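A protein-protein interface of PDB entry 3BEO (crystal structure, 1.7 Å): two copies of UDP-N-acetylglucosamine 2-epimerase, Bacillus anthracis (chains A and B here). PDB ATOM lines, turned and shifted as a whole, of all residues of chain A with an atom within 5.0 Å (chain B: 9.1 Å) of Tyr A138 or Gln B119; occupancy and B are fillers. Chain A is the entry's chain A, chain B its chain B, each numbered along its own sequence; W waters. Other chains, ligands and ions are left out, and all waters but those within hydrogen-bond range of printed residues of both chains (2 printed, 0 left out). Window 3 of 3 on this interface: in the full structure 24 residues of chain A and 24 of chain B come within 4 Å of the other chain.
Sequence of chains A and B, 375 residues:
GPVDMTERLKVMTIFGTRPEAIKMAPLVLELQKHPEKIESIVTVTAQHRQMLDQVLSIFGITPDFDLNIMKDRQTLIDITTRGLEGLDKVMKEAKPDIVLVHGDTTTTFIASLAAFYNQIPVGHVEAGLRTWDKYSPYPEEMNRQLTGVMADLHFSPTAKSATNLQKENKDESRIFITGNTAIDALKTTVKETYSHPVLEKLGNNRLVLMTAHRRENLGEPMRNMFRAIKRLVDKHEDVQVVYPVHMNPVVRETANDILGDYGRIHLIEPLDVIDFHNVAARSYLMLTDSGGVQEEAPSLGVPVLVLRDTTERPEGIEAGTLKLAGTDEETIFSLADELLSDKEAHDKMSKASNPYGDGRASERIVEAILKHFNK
The side-chain carboxylate (OD2) of Asp B152 is in salt-bridge range of the side-chain amino group (NZ) of Lys A134, at 2.7 Å.
The side-chain hydroxyl (OH) of Tyr A138 is in hydrogen-bond range of the backbone carbonyl oxygen (O) of Phe B116, 2.7 Å away.
The side-chain hydroxyl of Tyr A138 sits close to the backbone carbonyl oxygen of Tyr B117.
The side-chain carboxylate (OE1) of Glu A140 sits close to the backbone NH (N) of Tyr A138 (3.5 Å).
The backbone NH (N) of Tyr A138 sits at hydrogen-bond distance from the side-chain carboxylate (OE1) of Glu A216, at 3.0 Å.
O of Val B122 lies within hydrogen-bond range of N of Asp B152.
Leu A76 touches Tyr B117 (CD1 to CD1, 3.7 Å).
Lys A134 touches Phe B116.
Tyr A135 touches Gln B119.
Tyr A138 touches Gln B119 (CE2 to NE2, 3.5 Å).
Pro A139 touches Phe B116.
Printed residues of chain B within 4 Å of Leu A76: Tyr B117 (3.7 Å).
Of the printed residues of chain B, Lys A134 touches Phe B116 (3.4 Å) and Asp B152 (2.7 Å).
Of the printed residues of chain B, Tyr A135 touches Gln B119 (3.8 Å).
No residue of chain B comes within 4 Å of Pro A137.
Met B91 touches none of the printed residues of chain A.
Of the printed residues of chain A, Tyr B117 touches Leu A76 and Tyr A138.
Of the printed residues of chain A, Gln B119 touches Tyr A135 (3.8 Å) and Tyr A138 (3.5 Å).
The nearest residue of chain B that does not touch Tyr A138 is Asn B118 (4.04 Å).
The nearest printed residue of chain A that does not touch Gln B119 is Glu A216 (6.1 Å).
Of the 10 printed residues of chain A, 5 touch a printed residue of chain B.
Among the printed residues, Asp or Glu carboxylates within 4 Å of a Lys or Arg side-chain nitrogen of the other chain: Lys A134 with Asp B152 (2.7 Å).
No position is printed for both chains.
Of the 8 pairs that touch across the chains among the printed residues, none has its exchanged pair printed and touching as well.
Water W1 lies within hydrogen-bond range of the backbone carbonyl oxygen (O) of Ile B120 (2.6 Å), the side-chain hydroxyl (OH) of Tyr A135 (2.7 Å) and the side-chain amino group (NZ) of Lys A134 (2.9 Å).
Water W2 bridges the side-chain hydroxyl of Tyr A135 (2.7 Å) and the side-chain carboxylate of Asp B152 (2.8 Å).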
ATOM      1  N   LEU A  76       9.083  -7.659  21.118  1.00  0.00           N
ATOM      2  CA  LEU A  76       8.673  -9.042  20.812  1.00  0.00           C
ATOM      3  C   LEU A  76       9.459  -9.502  19.615  1.00  0.00           C
ATOM      4  O   LEU A  76       9.729 -10.703  19.486  1.00  0.00           O
ATOM      5  CB  LEU A  76       7.191  -9.095  20.506  1.00  0.00           C
ATOM      6  CG  LEU A  76       6.233  -8.800  21.677  1.00  0.00           C
ATOM      7  CD1 LEU A  76       4.814  -8.925  21.172  1.00  0.00           C
ATOM      8  CD2 LEU A  76       6.504  -9.818  22.842  1.00  0.00           C
ATOM      9  N   LYS A 134      -7.334 -12.448  21.731  1.00  0.00           N
ATOM     10  CA  LYS A 134      -5.921 -12.345  21.334  1.00  0.00           C
ATOM     11  C   LYS A 134      -5.215 -11.072  21.791  1.00  0.00           C
ATOM     12  O   LYS A 134      -4.022 -10.933  21.577  1.00  0.00           O
ATOM     13  CB  LYS A 134      -5.756 -12.521  19.832  1.00  0.00           C
ATOM     14  CG  LYS A 134      -6.259 -11.413  18.937  1.00  0.00           C
ATOM     15  CD  LYS A 134      -5.792 -11.724  17.496  1.00  0.00           C
ATOM     16  CE  LYS A 134      -6.329 -10.733  16.478  1.00  0.00           C
ATOM     17  NZ  LYS A 134      -5.663 -10.884  15.156  1.00  0.00           N
ATOM     18  N   TYR A 135      -5.960 -10.132  22.394  1.00  0.00           N
ATOM     19  CA  TYR A 135      -5.357  -8.956  23.015  1.00  0.00           C
ATOM     20  C   TYR A 135      -5.431  -8.935  24.562  1.00  0.00           C
ATOM     21  O   TYR A 135      -5.073  -7.942  25.211  1.00  0.00           O
ATOM     22  CB  TYR A 135      -5.927  -7.688  22.376  1.00  0.00           C
ATOM     23  CG  TYR A 135      -5.709  -7.632  20.868  1.00  0.00           C
ATOM     24  CD1 TYR A 135      -4.419  -7.814  20.321  1.00  0.00           C
ATOM     25  CD2 TYR A 135      -6.784  -7.457  20.000  1.00  0.00           C
ATOM     26  CE1 TYR A 135      -4.209  -7.790  18.931  1.00  0.00           C
ATOM     27  CE2 TYR A 135      -6.594  -7.374  18.619  1.00  0.00           C
ATOM     28  CZ  TYR A 135      -5.297  -7.556  18.092  1.00  0.00           C
ATOM     29  OH  TYR A 135      -5.158  -7.494  16.737  1.00  0.00           O
ATOM     30  N   SER A 136      -5.819 -10.058  25.158  1.00  0.00           N
ATOM     31  CA  SER A 136      -5.888 -10.195  26.599  1.00  0.00           C
ATOM     32  C   SER A 136      -5.881 -11.696  27.057  1.00  0.00           C
ATOM     33  O   SER A 136      -6.938 -12.357  27.093  1.00  0.00           O
ATOM     34  CB  SER A 136      -7.133  -9.504  27.169  1.00  0.00           C
ATOM     35  OG  SER A 136      -7.127  -9.640  28.576  1.00  0.00           O
ATOM     36  N   PRO A 137      -4.696 -12.220  27.416  1.00  0.00           N
ATOM     37  CA  PRO A 137      -3.360 -11.595  27.539  1.00  0.00           C
ATOM     38  C   PRO A 137      -2.704 -11.484  26.200  1.00  0.00           C
ATOM     39  O   PRO A 137      -2.921 -12.367  25.373  1.00  0.00           O
ATOM     40  CB  PRO A 137      -2.562 -12.571  28.416  1.00  0.00           C
ATOM     41  CG  PRO A 137      -3.295 -13.848  28.243  1.00  0.00           C
ATOM     42  CD  PRO A 137      -4.675 -13.615  27.849  1.00  0.00           C
ATOM     43  N   TYR A 138      -1.954 -10.390  26.026  1.00  0.00           N
ATOM     44  CA  TYR A 138      -1.166 -10.118  24.854  1.00  0.00           C
ATOM     45  C   TYR A 138       0.303 -10.091  25.198  1.00  0.00           C
ATOM     46  O   TYR A 138       0.704  -9.299  26.127  1.00  0.00           O
ATOM     47  CB  TYR A 138      -1.544  -8.771  24.294  1.00  0.00           C
ATOM     48  CG  TYR A 138      -0.798  -8.343  23.056  1.00  0.00           C
ATOM     49  CD1 TYR A 138      -1.228  -8.745  21.789  1.00  0.00           C
ATOM     50  CD2 TYR A 138       0.343  -7.512  23.153  1.00  0.00           C
ATOM     51  CE1 TYR A 138      -0.504  -8.354  20.628  1.00  0.00           C
ATOM     52  CE2 TYR A 138       1.016  -7.112  22.048  1.00  0.00           C
ATOM     53  CZ  TYR A 138       0.559  -7.501  20.776  1.00  0.00           C
ATOM     54  OH  TYR A 138       1.235  -7.087  19.678  1.00  0.00           O
ATOM     55  N   PRO A 139       1.110 -10.873  24.449  1.00  0.00           N
ATOM     56  CA  PRO A 139       0.794 -11.836  23.290  1.00  0.00           C
ATOM     57  C   PRO A 139       0.611 -13.356  23.671  1.00  0.00           C
ATOM     58  O   PRO A 139       0.588 -14.267  22.780  1.00  0.00           O
ATOM     59  CB  PRO A 139       2.080 -11.771  22.476  1.00  0.00           C
ATOM     60  CG  PRO A 139       3.139 -11.703  23.523  1.00  0.00           C
ATOM     61  CD  PRO A 139       2.568 -10.828  24.673  1.00  0.00           C
ATOM     62  N   GLU A 140       0.372 -13.602  24.957  1.00  0.00           N
ATOM     63  CA  GLU A 140       0.371 -14.977  25.516  1.00  0.00           C
ATOM     64  C   GLU A 140      -0.754 -15.813  24.978  1.00  0.00           C
ATOM     65  O   GLU A 140      -0.552 -16.974  24.739  1.00  0.00           O
ATOM     66  CB  GLU A 140       0.342 -14.959  27.050  1.00  0.00           C
ATOM     67  CG  GLU A 140       1.606 -14.383  27.709  1.00  0.00           C
ATOM     68  CD  GLU A 140       1.617 -12.849  27.918  1.00  0.00           C
ATOM     69  OE1 GLU A 140       0.747 -12.160  27.348  1.00  0.00           O
ATOM     70  OE2 GLU A 140       2.568 -12.365  28.597  1.00  0.00           O
ATOM     71  N   ARG A 215       1.543  -7.256  30.035  1.00  0.00           N
ATOM     72  CA  ARG A 215       1.905  -6.330  28.957  1.00  0.00           C
ATOM     73  C   ARG A 215       0.741  -5.365  28.667  1.00  0.00           C
ATOM     74  O   ARG A 215       0.954  -4.143  28.488  1.00  0.00           O
ATOM     75  CB  ARG A 215       2.296  -7.152  27.712  1.00  0.00           C
ATOM     76  CG  ARG A 215       2.959  -6.320  26.619  1.00  0.00           C
ATOM     77  CD  ARG A 215       3.577  -7.182  25.556  1.00  0.00           C
ATOM     78  NE  ARG A 215       4.535  -8.134  26.134  1.00  0.00           N
ATOM     79  CZ  ARG A 215       5.852  -8.111  25.944  1.00  0.00           C
ATOM     80  NH1 ARG A 215       6.385  -7.279  25.061  1.00  0.00           N
ATOM     81  NH2 ARG A 215       6.630  -8.973  26.575  1.00  0.00           N
ATOM     82  N   GLU A 216      -0.465  -5.900  28.603  1.00  0.00           N
ATOM     83  CA  GLU A 216      -1.656  -5.159  28.210  1.00  0.00           C
ATOM     84  C   GLU A 216      -2.115  -4.266  29.340  1.00  0.00           C
ATOM     85  O   GLU A 216      -2.983  -3.431  29.137  1.00  0.00           O
ATOM     86  CB  GLU A 216      -2.813  -6.088  27.809  1.00  0.00           C
ATOM     87  CG  GLU A 216      -3.356  -7.000  28.852  1.00  0.00           C
ATOM     88  CD  GLU A 216      -2.602  -8.308  29.028  1.00  0.00           C
ATOM     89  OE1 GLU A 216      -1.558  -8.523  28.324  1.00  0.00           O
ATOM     90  OE2 GLU A 216      -3.073  -9.094  29.941  1.00  0.00           O
ATOM     91  N   ASP B  88       7.674  -5.299  10.034  1.00  0.00           N
ATOM     92  CA  ASP B  88       7.386  -4.517  11.261  1.00  0.00           C
ATOM     93  C   ASP B  88       7.663  -3.071  10.936  1.00  0.00           C
ATOM     94  O   ASP B  88       6.917  -2.195  11.319  1.00  0.00           O
ATOM     95  CB  ASP B  88       8.243  -5.004  12.409  1.00  0.00           C
ATOM     96  CG  ASP B  88       7.994  -4.234  13.707  1.00  0.00           C
ATOM     97  OD1 ASP B  88       6.818  -4.219  14.116  1.00  0.00           O
ATOM     98  OD2 ASP B  88       8.956  -3.646  14.266  1.00  0.00           O
ATOM     99  N   MET B  91       4.882  -1.642   8.638  1.00  0.00           N
ATOM    100  CA  MET B  91       3.616  -1.463   9.349  1.00  0.00           C
ATOM    101  C   MET B  91       3.623  -0.270  10.302  1.00  0.00           C
ATOM    102  O   MET B  91       2.577   0.396  10.494  1.00  0.00           O
ATOM    103  CB  MET B  91       3.267  -2.760  10.070  1.00  0.00           C
ATOM    104  CG  MET B  91       2.845  -3.866   9.065  1.00  0.00           C
ATOM    105  SD  MET B  91       2.534  -5.386   9.926  1.00  0.00           S
ATOM    106  CE  MET B  91       2.334  -6.454   8.500  1.00  0.00           C
ATOM    107  N   LYS B  92       4.784   0.004  10.900  1.00  0.00           N
ATOM    108  CA  LYS B  92       4.943   1.127  11.826  1.00  0.00           C
ATOM    109  C   LYS B  92       4.924   2.448  11.050  1.00  0.00           C
ATOM    110  O   LYS B  92       4.503   3.490  11.605  1.00  0.00           O
ATOM    111  CB  LYS B  92       6.207   0.977  12.650  1.00  0.00           C
ATOM    112  CG  LYS B  92       6.007   0.020  13.862  1.00  0.00           C
ATOM    113  CD  LYS B  92       7.305  -0.249  14.576  1.00  0.00           C
ATOM    114  CE  LYS B  92       7.070  -0.819  16.017  1.00  0.00           C
ATOM    115  NZ  LYS B  92       6.421  -2.118  16.033  1.00  0.00           N
ATOM    116  N   LYS B  95       0.953   2.214   8.971  1.00  0.00           N
ATOM    117  CA  LYS B  95      -0.145   2.091   9.907  1.00  0.00           C
ATOM    118  C   LYS B  95      -1.489   1.705   9.248  1.00  0.00           C
ATOM    119  O   LYS B  95      -2.527   2.425   9.420  1.00  0.00           O
ATOM    120  CB  LYS B  95      -0.276   3.391  10.756  1.00  0.00           C
ATOM    121  CG  LYS B  95       0.917   3.637  11.638  1.00  0.00           C
ATOM    122  CD  LYS B  95       1.009   4.989  12.210  1.00  0.00           C
ATOM    123  CE  LYS B  95       2.128   5.047  13.262  1.00  0.00           C
ATOM    124  NZ  LYS B  95       2.174   6.384  13.973  1.00  0.00           N
ATOM    125  N   PRO B  96      -1.488   0.572   8.504  1.00  0.00           N
ATOM    126  CA  PRO B  96      -2.703   0.138   7.848  1.00  0.00           C
ATOM    127  C   PRO B  96      -3.791  -0.239   8.880  1.00  0.00           C
ATOM    128  O   PRO B  96      -3.450  -0.630  10.006  1.00  0.00           O
ATOM    129  CB  PRO B  96      -2.247  -1.109   7.043  1.00  0.00           C
ATOM    130  CG  PRO B  96      -1.104  -1.648   7.820  1.00  0.00           C
ATOM    131  CD  PRO B  96      -0.394  -0.408   8.325  1.00  0.00           C
ATOM    132  N   ASP B  97      -5.055  -0.141   8.475  1.00  0.00           N
ATOM    133  CA  ASP B  97      -6.223  -0.613   9.203  1.00  0.00           C
ATOM    134  C   ASP B  97      -6.389  -2.143   9.184  1.00  0.00           C
ATOM    135  O   ASP B  97      -6.949  -2.758  10.130  1.00  0.00           O
ATOM    136  CB  ASP B  97      -7.484   0.123   8.694  1.00  0.00           C
ATOM    137  CG  ASP B  97      -7.378   1.664   8.889  1.00  0.00           C
ATOM    138  OD1 ASP B  97      -7.149   2.114  10.064  1.00  0.00           O
ATOM    139  OD2 ASP B  97      -7.488   2.437   7.897  1.00  0.00           O
ATOM    140  N   ILE B  98      -5.928  -2.775   8.093  1.00  0.00           N
ATOM    141  CA  ILE B  98      -6.013  -4.201   7.986  1.00  0.00           C
ATOM    142  C   ILE B  98      -4.915  -4.684   7.040  1.00  0.00           C
ATOM    143  O   ILE B  98      -4.555  -3.968   6.163  1.00  0.00           O
ATOM    144  CB  ILE B  98      -7.407  -4.665   7.498  1.00  0.00           C
ATOM    145  CG1 ILE B  98      -7.501  -6.210   7.498  1.00  0.00           C
ATOM    146  CG2 ILE B  98      -7.769  -4.135   6.086  1.00  0.00           C
ATOM    147  CD1 ILE B  98      -8.942  -6.680   7.309  1.00  0.00           C
ATOM    148  N   VAL B  99      -4.339  -5.832   7.362  1.00  0.00           N
ATOM    149  CA  VAL B  99      -3.363  -6.514   6.525  1.00  0.00           C
ATOM    150  C   VAL B  99      -4.008  -7.772   5.946  1.00  0.00           C
ATOM    151  O   VAL B  99      -4.596  -8.587   6.680  1.00  0.00           O
ATOM    152  CB  VAL B  99      -2.083  -6.880   7.385  1.00  0.00           C
ATOM    153  CG1 VAL B  99      -1.204  -7.851   6.700  1.00  0.00           C
ATOM    154  CG2 VAL B  99      -1.340  -5.627   7.794  1.00  0.00           C
ATOM    155  N   SER B 112       1.361 -12.116   8.917  1.00  0.00           N
ATOM    156  CA  SER B 112       0.358 -12.243   9.976  1.00  0.00           C
ATOM    157  C   SER B 112       0.930 -11.966  11.338  1.00  0.00           C
ATOM    158  O   SER B 112       0.316 -11.268  12.130  1.00  0.00           O
ATOM    159  CB  SER B 112      -0.280 -13.614   9.931  1.00  0.00           C
ATOM    160  OG  SER B 112      -0.960 -13.745   8.698  1.00  0.00           O
ATOM    161  N   LEU B 113       2.138 -12.489  11.590  1.00  0.00           N
ATOM    162  CA  LEU B 113       2.825 -12.289  12.870  1.00  0.00           C
ATOM    163  C   LEU B 113       3.190 -10.814  13.086  1.00  0.00           C
ATOM    164  O   LEU B 113       2.913 -10.237  14.136  1.00  0.00           O
ATOM    165  CB  LEU B 113       4.085 -13.147  12.989  1.00  0.00           C
ATOM    166  CG  LEU B 113       4.719 -13.303  14.366  1.00  0.00           C
ATOM    167  CD1 LEU B 113       3.739 -14.023  15.356  1.00  0.00           C
ATOM    168  CD2 LEU B 113       6.017 -14.036  14.306  1.00  0.00           C
ATOM    169  N   ALA B 114       3.750 -10.182  12.052  1.00  0.00           N
ATOM    170  CA  ALA B 114       4.120  -8.755  12.144  1.00  0.00           C
ATOM    171  C   ALA B 114       2.833  -7.921  12.416  1.00  0.00           C
ATOM    172  O   ALA B 114       2.882  -7.003  13.208  1.00  0.00           O
ATOM    173  CB  ALA B 114       4.800  -8.277  10.903  1.00  0.00           C
ATOM    174  N   ALA B 115       1.724  -8.214  11.724  1.00  0.00           N
ATOM    175  CA  ALA B 115       0.434  -7.505  11.964  1.00  0.00           C
ATOM    176  C   ALA B 115       0.040  -7.667  13.438  1.00  0.00           C
ATOM    177  O   ALA B 115      -0.270  -6.706  14.130  1.00  0.00           O
ATOM    178  CB  ALA B 115      -0.720  -8.025  10.989  1.00  0.00           C
ATOM    179  N   PHE B 116       0.121  -8.886  13.943  1.00  0.00           N
ATOM    180  CA  PHE B 116      -0.262  -9.168  15.321  1.00  0.00           C
ATOM    181  C   PHE B 116       0.611  -8.420  16.302  1.00  0.00           C
ATOM    182  O   PHE B 116       0.121  -7.884  17.337  1.00  0.00           O
ATOM    183  CB  PHE B 116      -0.178 -10.680  15.558  1.00  0.00           C
ATOM    184  CG  PHE B 116      -0.424 -11.066  17.005  1.00  0.00           C
ATOM    185  CD1 PHE B 116      -1.678 -10.839  17.588  1.00  0.00           C
ATOM    186  CD2 PHE B 116       0.593 -11.585  17.791  1.00  0.00           C
ATOM    187  CE1 PHE B 116      -1.879 -11.201  18.889  1.00  0.00           C
ATOM    188  CE2 PHE B 116       0.378 -11.890  19.139  1.00  0.00           C
ATOM    189  CZ  PHE B 116      -0.863 -11.671  19.679  1.00  0.00           C
ATOM    190  N   TYR B 117       1.914  -8.370  16.010  1.00  0.00           N
ATOM    191  CA  TYR B 117       2.866  -7.629  16.840  1.00  0.00           C
ATOM    192  C   TYR B 117       2.678  -6.112  16.789  1.00  0.00           C
ATOM    193  O   TYR B 117       3.360  -5.418  17.537  1.00  0.00           O
ATOM    194  CB  TYR B 117       4.271  -7.990  16.403  1.00  0.00           C
ATOM    195  CG  TYR B 117       4.772  -9.311  16.885  1.00  0.00           C
ATOM    196  CD1 TYR B 117       4.073 -10.107  17.781  1.00  0.00           C
ATOM    197  CD2 TYR B 117       6.033  -9.741  16.502  1.00  0.00           C
ATOM    198  CE1 TYR B 117       4.618 -11.321  18.263  1.00  0.00           C
ATOM    199  CE2 TYR B 117       6.549 -10.945  16.945  1.00  0.00           C
ATOM    200  CZ  TYR B 117       5.826 -11.722  17.825  1.00  0.00           C
ATOM    201  OH  TYR B 117       6.410 -12.880  18.256  1.00  0.00           O
ATOM    202  N   ASN B 118       1.770  -5.653  15.938  1.00  0.00           N
ATOM    203  CA  ASN B 118       1.373  -4.242  15.765  1.00  0.00           C
ATOM    204  C   ASN B 118      -0.161  -4.043  16.036  1.00  0.00           C
ATOM    205  O   ASN B 118      -0.721  -2.985  15.745  1.00  0.00           O
ATOM    206  CB  ASN B 118       1.787  -3.757  14.363  1.00  0.00           C
ATOM    207  CG  ASN B 118       3.252  -3.445  14.287  1.00  0.00           C
ATOM    208  OD1 ASN B 118       3.727  -2.415  14.825  1.00  0.00           O
ATOM    209  ND2 ASN B 118       4.002  -4.351  13.708  1.00  0.00           N
ATOM    210  N   GLN B 119      -0.809  -5.072  16.557  1.00  0.00           N
ATOM    211  CA  GLN B 119      -2.233  -5.111  16.836  1.00  0.00           C
ATOM    212  C   GLN B 119      -3.041  -4.599  15.598  1.00  0.00           C
ATOM    213  O   GLN B 119      -3.971  -3.811  15.687  1.00  0.00           O
ATOM    214  CB  GLN B 119      -2.491  -4.330  18.141  1.00  0.00           C
ATOM    215  CG  GLN B 119      -1.753  -4.968  19.356  1.00  0.00           C
ATOM    216  CD  GLN B 119      -2.270  -4.492  20.725  1.00  0.00           C
ATOM    217  OE1 GLN B 119      -3.031  -3.535  20.799  1.00  0.00           O
ATOM    218  NE2 GLN B 119      -1.835  -5.158  21.815  1.00  0.00           N
ATOM    219  N   ILE B 120      -2.671  -5.116  14.432  1.00  0.00           N
ATOM    220  CA  ILE B 120      -3.393  -4.790  13.220  1.00  0.00           C
ATOM    221  C   ILE B 120      -4.169  -6.055  12.804  1.00  0.00           C
ATOM    222  O   ILE B 120      -3.582  -7.167  12.798  1.00  0.00           O
ATOM    223  CB  ILE B 120      -2.455  -4.353  12.061  1.00  0.00           C
ATOM    224  CG1 ILE B 120      -1.483  -3.254  12.511  1.00  0.00           C
ATOM    225  CG2 ILE B 120      -3.263  -4.021  10.790  1.00  0.00           C
ATOM    226  CD1 ILE B 120      -0.341  -2.932  11.586  1.00  0.00           C
ATOM    227  N   PRO B 121      -5.482  -5.903  12.470  1.00  0.00           N
ATOM    228  CA  PRO B 121      -6.274  -7.059  12.025  1.00  0.00           C
ATOM    229  C   PRO B 121      -5.729  -7.689  10.716  1.00  0.00           C
ATOM    230  O   PRO B 121      -5.181  -7.020   9.868  1.00  0.00           O
ATOM    231  CB  PRO B 121      -7.681  -6.496  11.785  1.00  0.00           C
ATOM    232  CG  PRO B 121      -7.721  -5.170  12.436  1.00  0.00           C
ATOM    233  CD  PRO B 121      -6.302  -4.675  12.492  1.00  0.00           C
ATOM    234  N   VAL B 122      -5.965  -8.973  10.573  1.00  0.00           N
ATOM    235  CA  VAL B 122      -5.490  -9.765   9.490  1.00  0.00           C
ATOM    236  C   VAL B 122      -6.690 -10.433   8.816  1.00  0.00           C
ATOM    237  O   VAL B 122      -7.519 -11.096   9.472  1.00  0.00           O
ATOM    238  CB  VAL B 122      -4.483 -10.864  10.038  1.00  0.00           C
ATOM    239  CG1 VAL B 122      -4.141 -11.922   8.927  1.00  0.00           C
ATOM    240  CG2 VAL B 122      -3.203 -10.150  10.609  1.00  0.00           C
ATOM    241  N   ASP B 152      -8.209 -12.515  11.718  1.00  0.00           N
ATOM    242  CA  ASP B 152      -9.505 -12.011  12.125  1.00  0.00           C
ATOM    243  C   ASP B 152     -10.649 -12.334  11.150  1.00  0.00           C
ATOM    244  O   ASP B 152     -11.793 -12.426  11.583  1.00  0.00           O
ATOM    245  CB  ASP B 152      -9.443 -10.481  12.317  1.00  0.00           C
ATOM    246  CG  ASP B 152      -8.436 -10.066  13.358  1.00  0.00           C
ATOM    247  OD1 ASP B 152      -8.858  -9.827  14.511  1.00  0.00           O
ATOM    248  OD2 ASP B 152      -7.232 -10.000  13.088  1.00  0.00           O
ATOM    249  N   PHE B 373     -15.712  -3.269   8.599  1.00  0.00           N
ATOM    250  CA  PHE B 373     -15.316  -2.016   9.179  1.00  0.00           C
ATOM    251  C   PHE B 373     -16.465  -0.986   9.081  1.00  0.00           C
ATOM    252  O   PHE B 373     -16.289   0.164   9.469  1.00  0.00           O
ATOM    253  CB  PHE B 373     -14.049  -1.496   8.502  1.00  0.00           C
ATOM    254  CG  PHE B 373     -12.770  -2.198   8.937  1.00  0.00           C
ATOM    255  CD1 PHE B 373     -12.117  -1.825  10.144  1.00  0.00           C
ATOM    256  CD2 PHE B 373     -12.194  -3.170   8.136  1.00  0.00           C
ATOM    257  CE1 PHE B 373     -10.971  -2.444  10.526  1.00  0.00           C
ATOM    258  CE2 PHE B 373     -11.051  -3.834   8.552  1.00  0.00           C
ATOM    259  CZ  PHE B 373     -10.423  -3.431   9.709  1.00  0.00           C
HETATM  260  O   HOH W   1      -3.718  -8.811  14.818  1.00  0.00           O
HETATM  261  O   HOH W   2      -7.568  -7.554  15.424  1.00  0.00           O
